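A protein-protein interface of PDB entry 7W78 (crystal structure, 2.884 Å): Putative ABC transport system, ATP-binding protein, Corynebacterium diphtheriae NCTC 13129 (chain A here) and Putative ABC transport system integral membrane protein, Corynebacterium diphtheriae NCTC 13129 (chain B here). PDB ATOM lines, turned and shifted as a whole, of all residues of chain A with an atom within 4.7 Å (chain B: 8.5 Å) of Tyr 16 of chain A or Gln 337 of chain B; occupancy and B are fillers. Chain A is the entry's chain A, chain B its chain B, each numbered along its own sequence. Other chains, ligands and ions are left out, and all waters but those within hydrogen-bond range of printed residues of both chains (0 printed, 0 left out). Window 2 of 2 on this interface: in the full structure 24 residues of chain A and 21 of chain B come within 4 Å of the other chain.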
ATOM      1  N   VAL A  14     -26.024  22.208  29.509  1.00  0.00           N
ATOM      2  CA  VAL A  14     -26.071  21.319  28.350  1.00  0.00           C
ATOM      3  C   VAL A  14     -24.971  20.280  28.503  1.00  0.00           C
ATOM      4  O   VAL A  14     -23.799  20.629  28.679  1.00  0.00           O
ATOM      5  CB  VAL A  14     -25.912  22.076  27.019  1.00  0.00           C
ATOM      6  CG1 VAL A  14     -26.060  21.109  25.855  1.00  0.00           C
ATOM      7  CG2 VAL A  14     -26.932  23.198  26.910  1.00  0.00           C
ATOM      8  N   VAL A  15     -25.348  19.007  28.431  1.00  0.00           N
ATOM      9  CA  VAL A  15     -24.421  17.890  28.580  1.00  0.00           C
ATOM     10  C   VAL A  15     -24.577  16.994  27.359  1.00  0.00           C
ATOM     11  O   VAL A  15     -25.684  16.522  27.070  1.00  0.00           O
ATOM     12  CB  VAL A  15     -24.676  17.103  29.875  1.00  0.00           C
ATOM     13  CG1 VAL A  15     -23.576  16.093  30.107  1.00  0.00           C
ATOM     14  CG2 VAL A  15     -24.782  18.043  31.068  1.00  0.00           C
ATOM     15  N   TYR A  16     -23.472  16.767  26.637  1.00  0.00           N
ATOM     16  CA  TYR A  16     -23.474  15.875  25.488  1.00  0.00           C
ATOM     17  C   TYR A  16     -22.777  14.559  25.822  1.00  0.00           C
ATOM     18  O   TYR A  16     -21.845  14.531  26.631  1.00  0.00           O
ATOM     19  CB  TYR A  16     -22.774  16.496  24.274  1.00  0.00           C
ATOM     20  CG  TYR A  16     -23.358  17.800  23.794  1.00  0.00           C
ATOM     21  CD1 TYR A  16     -24.663  17.875  23.326  1.00  0.00           C
ATOM     22  CD2 TYR A  16     -22.590  18.955  23.779  1.00  0.00           C
ATOM     23  CE1 TYR A  16     -25.191  19.072  22.873  1.00  0.00           C
ATOM     24  CE2 TYR A  16     -23.103  20.150  23.324  1.00  0.00           C
ATOM     25  CZ  TYR A  16     -24.404  20.204  22.874  1.00  0.00           C
ATOM     26  OH  TYR A  16     -24.922  21.397  22.426  1.00  0.00           O
ATOM     27  N   PRO A  17     -23.209  13.453  25.213  1.00  0.00           N
ATOM     28  CA  PRO A  17     -22.508  12.175  25.410  1.00  0.00           C
ATOM     29  C   PRO A  17     -21.291  12.068  24.499  1.00  0.00           C
ATOM     30  O   PRO A  17     -21.389  12.262  23.284  1.00  0.00           O
ATOM     31  CB  PRO A  17     -23.570  11.131  25.044  1.00  0.00           C
ATOM     32  CG  PRO A  17     -24.445  11.836  24.054  1.00  0.00           C
ATOM     33  CD  PRO A  17     -24.474  13.285  24.473  1.00  0.00           C
ATOM     34  N   ASP A  18     -20.144  11.754  25.090  1.00  0.00           N
ATOM     35  CA  ASP A  18     -18.908  11.552  24.329  1.00  0.00           C
ATOM     36  C   ASP A  18     -18.554  10.065  24.277  1.00  0.00           C
ATOM     37  O   ASP A  18     -17.492   9.623  24.724  1.00  0.00           O
ATOM     38  CB  ASP A  18     -17.771  12.371  24.932  1.00  0.00           C
ATOM     39  CG  ASP A  18     -16.572  12.467  24.003  1.00  0.00           C
ATOM     40  OD1 ASP A  18     -15.481  12.856  24.471  1.00  0.00           O
ATOM     41  OD2 ASP A  18     -16.721  12.146  22.805  1.00  0.00           O
ATOM     42  N   THR A  22     -18.998  11.824  28.963  1.00  0.00           N
ATOM     43  CA  THR A  22     -19.929  12.883  28.612  1.00  0.00           C
ATOM     44  C   THR A  22     -19.182  14.207  28.689  1.00  0.00           C
ATOM     45  O   THR A  22     -18.192  14.330  29.414  1.00  0.00           O
ATOM     46  CB  THR A  22     -21.158  12.867  29.542  1.00  0.00           C
ATOM     47  OG1 THR A  22     -22.250  13.568  28.930  1.00  0.00           O
ATOM     48  CG2 THR A  22     -20.832  13.491  30.895  1.00  0.00           C
ATOM     49  N   VAL A  23     -19.637  15.188  27.911  1.00  0.00           N
ATOM     50  CA  VAL A  23     -19.014  16.508  27.863  1.00  0.00           C
ATOM     51  C   VAL A  23     -20.036  17.539  28.321  1.00  0.00           C
ATOM     52  O   VAL A  23     -21.166  17.560  27.822  1.00  0.00           O
ATOM     53  CB  VAL A  23     -18.492  16.849  26.454  1.00  0.00           C
ATOM     54  CG1 VAL A  23     -17.971  18.283  26.413  1.00  0.00           C
ATOM     55  CG2 VAL A  23     -17.404  15.877  26.030  1.00  0.00           C
ATOM     56  N   ALA A  25     -20.933  20.973  28.006  1.00  0.00           N
ATOM     57  CA  ALA A  25     -20.668  22.151  27.184  1.00  0.00           C
ATOM     58  C   ALA A  25     -21.008  23.442  27.920  1.00  0.00           C
ATOM     59  O   ALA A  25     -20.331  24.461  27.745  1.00  0.00           O
ATOM     60  CB  ALA A  25     -21.452  22.059  25.875  1.00  0.00           C
ATOM     61  N   THR A  51     -23.031  27.576  22.646  1.00  0.00           N
ATOM     62  CA  THR A  51     -23.955  26.734  23.396  1.00  0.00           C
ATOM     63  C   THR A  51     -24.932  27.582  24.199  1.00  0.00           C
ATOM     64  O   THR A  51     -26.121  27.250  24.291  1.00  0.00           O
ATOM     65  CB  THR A  51     -23.181  25.789  24.314  1.00  0.00           C
ATOM     66  OG1 THR A  51     -22.100  25.197  23.584  1.00  0.00           O
ATOM     67  CG2 THR A  51     -24.091  24.686  24.831  1.00  0.00           C
ATOM     68  N   SER A  54     -27.444  28.860  21.789  1.00  0.00           N
ATOM     69  CA  SER A  54     -28.292  27.809  21.234  1.00  0.00           C
ATOM     70  C   SER A  54     -29.517  27.570  22.106  1.00  0.00           C
ATOM     71  O   SER A  54     -30.613  27.321  21.590  1.00  0.00           O
ATOM     72  CB  SER A  54     -27.496  26.517  21.070  1.00  0.00           C
ATOM     73  OG  SER A  54     -27.308  25.877  22.318  1.00  0.00           O
ATOM     74  N   LEU A  59     -32.923  26.688  20.050  1.00  0.00           N
ATOM     75  CA  LEU A  59     -32.457  25.691  19.091  1.00  0.00           C
ATOM     76  C   LEU A  59     -32.409  24.304  19.716  1.00  0.00           C
ATOM     77  O   LEU A  59     -32.513  23.299  19.004  1.00  0.00           O
ATOM     78  CB  LEU A  59     -31.084  26.084  18.547  1.00  0.00           C
ATOM     79  CG  LEU A  59     -31.004  27.419  17.804  1.00  0.00           C
ATOM     80  CD1 LEU A  59     -29.581  27.696  17.347  1.00  0.00           C
ATOM     81  CD2 LEU A  59     -31.964  27.432  16.626  1.00  0.00           C
ATOM     82  N   GLN A  60     -32.253  24.230  21.036  1.00  0.00           N
ATOM     83  CA  GLN A  60     -32.349  22.979  21.770  1.00  0.00           C
ATOM     84  C   GLN A  60     -32.835  23.288  23.176  1.00  0.00           C
ATOM     85  O   GLN A  60     -32.612  24.384  23.698  1.00  0.00           O
ATOM     86  CB  GLN A  60     -31.009  22.232  21.834  1.00  0.00           C
ATOM     87  CG  GLN A  60     -29.884  23.008  22.498  1.00  0.00           C
ATOM     88  CD  GLN A  60     -28.614  22.189  22.634  1.00  0.00           C
ATOM     89  OE1 GLN A  60     -28.663  20.973  22.812  1.00  0.00           O
ATOM     90  NE2 GLN A  60     -27.467  22.853  22.548  1.00  0.00           N
ATOM     91  N   ALA B 254     -33.192  22.220   7.871  1.00  0.00           N
ATOM     92  CA  ALA B 254     -32.722  22.503   9.224  1.00  0.00           C
ATOM     93  C   ALA B 254     -32.542  24.000   9.451  1.00  0.00           C
ATOM     94  O   ALA B 254     -32.897  24.519  10.515  1.00  0.00           O
ATOM     95  CB  ALA B 254     -31.411  21.766   9.495  1.00  0.00           C
ATOM     96  N   ALA B 257     -35.934  25.629   9.730  1.00  0.00           N
ATOM     97  CA  ALA B 257     -36.496  25.285  11.033  1.00  0.00           C
ATOM     98  C   ALA B 257     -35.895  26.155  12.129  1.00  0.00           C
ATOM     99  O   ALA B 257     -36.616  26.676  12.987  1.00  0.00           O
ATOM    100  CB  ALA B 257     -36.262  23.805  11.333  1.00  0.00           C
ATOM    101  N   ALA B 258     -34.570  26.329  12.107  1.00  0.00           N
ATOM    102  CA  ALA B 258     -33.912  27.134  13.133  1.00  0.00           C
ATOM    103  C   ALA B 258     -34.447  28.560  13.147  1.00  0.00           C
ATOM    104  O   ALA B 258     -34.618  29.156  14.217  1.00  0.00           O
ATOM    105  CB  ALA B 258     -32.397  27.130  12.920  1.00  0.00           C
ATOM    106  N   VAL B 331     -36.481  14.977   9.671  1.00  0.00           N
ATOM    107  CA  VAL B 331     -35.640  16.131   9.981  1.00  0.00           C
ATOM    108  C   VAL B 331     -36.328  17.066  10.965  1.00  0.00           C
ATOM    109  O   VAL B 331     -35.708  17.530  11.926  1.00  0.00           O
ATOM    110  CB  VAL B 331     -35.263  16.864   8.681  1.00  0.00           C
ATOM    111  CG1 VAL B 331     -34.615  18.205   8.989  1.00  0.00           C
ATOM    112  CG2 VAL B 331     -34.341  16.009   7.868  1.00  0.00           C
ATOM    113  N   VAL B 334     -36.649  16.473  15.049  1.00  0.00           N
ATOM    114  CA  VAL B 334     -35.586  16.727  16.012  1.00  0.00           C
ATOM    115  C   VAL B 334     -35.494  18.217  16.304  1.00  0.00           C
ATOM    116  O   VAL B 334     -35.842  19.062  15.469  1.00  0.00           O
ATOM    117  CB  VAL B 334     -34.241  16.178  15.489  1.00  0.00           C
ATOM    118  CG1 VAL B 334     -33.223  16.116  16.607  1.00  0.00           C
ATOM    119  CG2 VAL B 334     -34.435  14.818  14.848  1.00  0.00           C
ATOM    120  N   ASP B 335     -35.040  18.541  17.513  1.00  0.00           N
ATOM    121  CA  ASP B 335     -34.656  19.909  17.822  1.00  0.00           C
ATOM    122  C   ASP B 335     -33.688  20.417  16.755  1.00  0.00           C
ATOM    123  O   ASP B 335     -32.787  19.676  16.335  1.00  0.00           O
ATOM    124  CB  ASP B 335     -34.009  19.988  19.208  1.00  0.00           C
ATOM    125  CG  ASP B 335     -35.020  19.873  20.334  1.00  0.00           C
ATOM    126  OD1 ASP B 335     -36.225  20.083  20.076  1.00  0.00           O
ATOM    127  OD2 ASP B 335     -34.609  19.591  21.479  1.00  0.00           O
ATOM    128  N   PRO B 336     -33.850  21.654  16.280  1.00  0.00           N
ATOM    129  CA  PRO B 336     -33.050  22.101  15.125  1.00  0.00           C
ATOM    130  C   PRO B 336     -31.547  22.092  15.360  1.00  0.00           C
ATOM    131  O   PRO B 336     -30.787  21.971  14.390  1.00  0.00           O
ATOM    132  CB  PRO B 336     -33.577  23.521  14.860  1.00  0.00           C
ATOM    133  CG  PRO B 336     -34.363  23.903  16.087  1.00  0.00           C
ATOM    134  CD  PRO B 336     -34.881  22.630  16.662  1.00  0.00           C
ATOM    135  N   GLN B 337     -31.090  22.207  16.612  1.00  0.00           N
ATOM    136  CA  GLN B 337     -29.654  22.194  16.875  1.00  0.00           C
ATOM    137  C   GLN B 337     -29.022  20.878  16.440  1.00  0.00           C
ATOM    138  O   GLN B 337     -27.891  20.859  15.941  1.00  0.00           O
ATOM    139  CB  GLN B 337     -29.387  22.455  18.360  1.00  0.00           C
ATOM    140  CG  GLN B 337     -27.981  22.072  18.834  1.00  0.00           C
ATOM    141  CD  GLN B 337     -26.943  23.155  18.577  1.00  0.00           C
ATOM    142  OE1 GLN B 337     -27.243  24.196  17.994  1.00  0.00           O
ATOM    143  NE2 GLN B 337     -25.714  22.909  19.014  1.00  0.00           N
ATOM    144  N   ILE B 338     -29.742  19.766  16.603  1.00  0.00           N
ATOM    145  CA  ILE B 338     -29.193  18.475  16.195  1.00  0.00           C
ATOM    146  C   ILE B 338     -29.178  18.356  14.678  1.00  0.00           C
ATOM    147  O   ILE B 338     -28.209  17.857  14.092  1.00  0.00           O
ATOM    148  CB  ILE B 338     -29.978  17.322  16.842  1.00  0.00           C
ATOM    149  CG1 ILE B 338     -29.942  17.436  18.366  1.00  0.00           C
ATOM    150  CG2 ILE B 338     -29.425  15.970  16.396  1.00  0.00           C
ATOM    151  CD1 ILE B 338     -28.536  17.331  18.947  1.00  0.00           C
ATOM    152  N   ALA B 339     -30.239  18.826  14.015  1.00  0.00           N
ATOM    153  CA  ALA B 339     -30.270  18.805  12.556  1.00  0.00           C
ATOM    154  C   ALA B 339     -29.136  19.636  11.971  1.00  0.00           C
ATOM    155  O   ALA B 339     -28.473  19.213  11.017  1.00  0.00           O
ATOM    156  CB  ALA B 339     -31.623  19.302  12.050  1.00  0.00           C
ATOM    157  N   LEU B 340     -28.882  20.814  12.547  1.00  0.00           N
ATOM    158  CA  LEU B 340     -27.743  21.618  12.120  1.00  0.00           C
ATOM    159  C   LEU B 340     -26.415  20.936  12.415  1.00  0.00           C
ATOM    160  O   LEU B 340     -25.391  21.322  11.840  1.00  0.00           O
ATOM    161  CB  LEU B 340     -27.778  22.986  12.798  1.00  0.00           C
ATOM    162  CG  LEU B 340     -28.917  23.902  12.357  1.00  0.00           C
ATOM    163  CD1 LEU B 340     -28.890  25.201  13.140  1.00  0.00           C
ATOM    164  CD2 LEU B 340     -28.823  24.164  10.867  1.00  0.00           C
ATOM    165  N   GLY B 341     -26.408  19.943  13.301  1.00  0.00           N
ATOM    166  CA  GLY B 341     -25.201  19.208  13.625  1.00  0.00           C
ATOM    167  C   GLY B 341     -24.937  18.071  12.663  1.00  0.00           C
ATOM    168  O   GLY B 341     -23.809  17.895  12.191  1.00  0.00           O
ATOM    169  N   ALA B 342     -25.977  17.289  12.361  1.00  0.00           N
ATOM    170  CA  ALA B 342     -25.849  16.226  11.371  1.00  0.00           C
ATOM    171  C   ALA B 342     -25.378  16.755  10.022  1.00  0.00           C
ATOM    172  O   ALA B 342     -24.910  15.974   9.187  1.00  0.00           O
ATOM    173  CB  ALA B 342     -27.180  15.489  11.217  1.00  0.00           C
ATOM    174  N   THR B 343     -25.502  18.058   9.790  1.00  0.00           N
ATOM    175  CA  THR B 343     -24.892  18.721   8.651  1.00  0.00           C
ATOM    176  C   THR B 343     -23.533  19.285   9.047  1.00  0.00           C
ATOM    177  O   THR B 343     -23.304  19.656  10.201  1.00  0.00           O
ATOM    178  CB  THR B 343     -25.790  19.843   8.133  1.00  0.00           C
ATOM    179  OG1 THR B 343     -25.594  21.016   8.930  1.00  0.00           O
ATOM    180  CG2 THR B 343     -27.240  19.427   8.221  1.00  0.00           C
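The backbone NH of Gln 337 of chain B sits at hydrogen-bond distance from the backbone carbonyl oxygen of Leu 59 of chain A, 3.0 Å away.
The backbone carbonyl oxygen of Leu 59 of chain A lies close to the backbone nitrogen of Pro 336 of chain B (3.5 Å).
The backbone carbonyl oxygen (O) of Tyr 16 of chain A lies within hydrogen-bond range of the side-chain hydroxyl (OG1) of Thr 22 of chain A.
The backbone carbonyl oxygen of Tyr 16 of chain A is in hydrogen-bond range of the backbone NH of Val 23 of chain A (2.6 Å).
The side-chain hydroxyl (OH) of Tyr 16 of chain A sits at hydrogen-bond distance from the side-chain amide nitrogen (NE2) of Gln 60 of chain A (2.9 Å).
The side-chain hydroxyl (OG) of Ser 54 of chain A lies within hydrogen-bond range of the backbone carbonyl oxygen (O) of Thr 51 of chain A, at 2.7 Å.
The backbone NH (N) of Leu 59 of chain A sits at hydrogen-bond distance from the backbone carbonyl oxygen (O) of Ser 54 of chain A (2.8 Å).
The side-chain hydroxyl (OG) of Ser 54 of chain A lies within hydrogen-bond range of the side-chain amide nitrogen (NE2) of Gln 60 of chain A, 3.0 Å away.
Of the 12 printed residues of chain A, 4 touch a printed residue of chain B.
Hydrophobic or aromatic side chains of chain B within 4 Å of the printed part of chain A: Ala 258 and Pro 336.
Among the printed residues, no Asp or Glu carboxylate lies within 4 Å of a Lys or Arg side-chain nitrogen of the other chain.
Tyr 16 of chain A touches just one residue of chain B: Gln 337.
Gln 337 of chain B touches four residues of chain A.
No residue of chain B comes within 4 Å of Pro 17 of chain A.
Of the printed residues of chain A, Asp 335 of chain B touches Leu 59 (3.6 Å).
Printed residues of chain A within 4 Å of Ala 258 of chain B: Leu 59 (3.7 Å).
The nearest residue of chain B that does not touch Tyr 16 of chain A is Ile 338 of chain B (5.4 Å).
Among the printed residues, merely in contact across the chains: Tyr 16 of chain A with Gln 337 of chain B (3.8 Å), Ser 54 of chain A with Gln 337 of chain B (3.9 Å), Leu 59 of chain A with Ala 258 of chain B (3.7 Å), Leu 59 of chain A with Asp 335 of chain B (3.6 Å) and Gln 60 of chain A with Gln 337 of chain B (3.8 Å).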
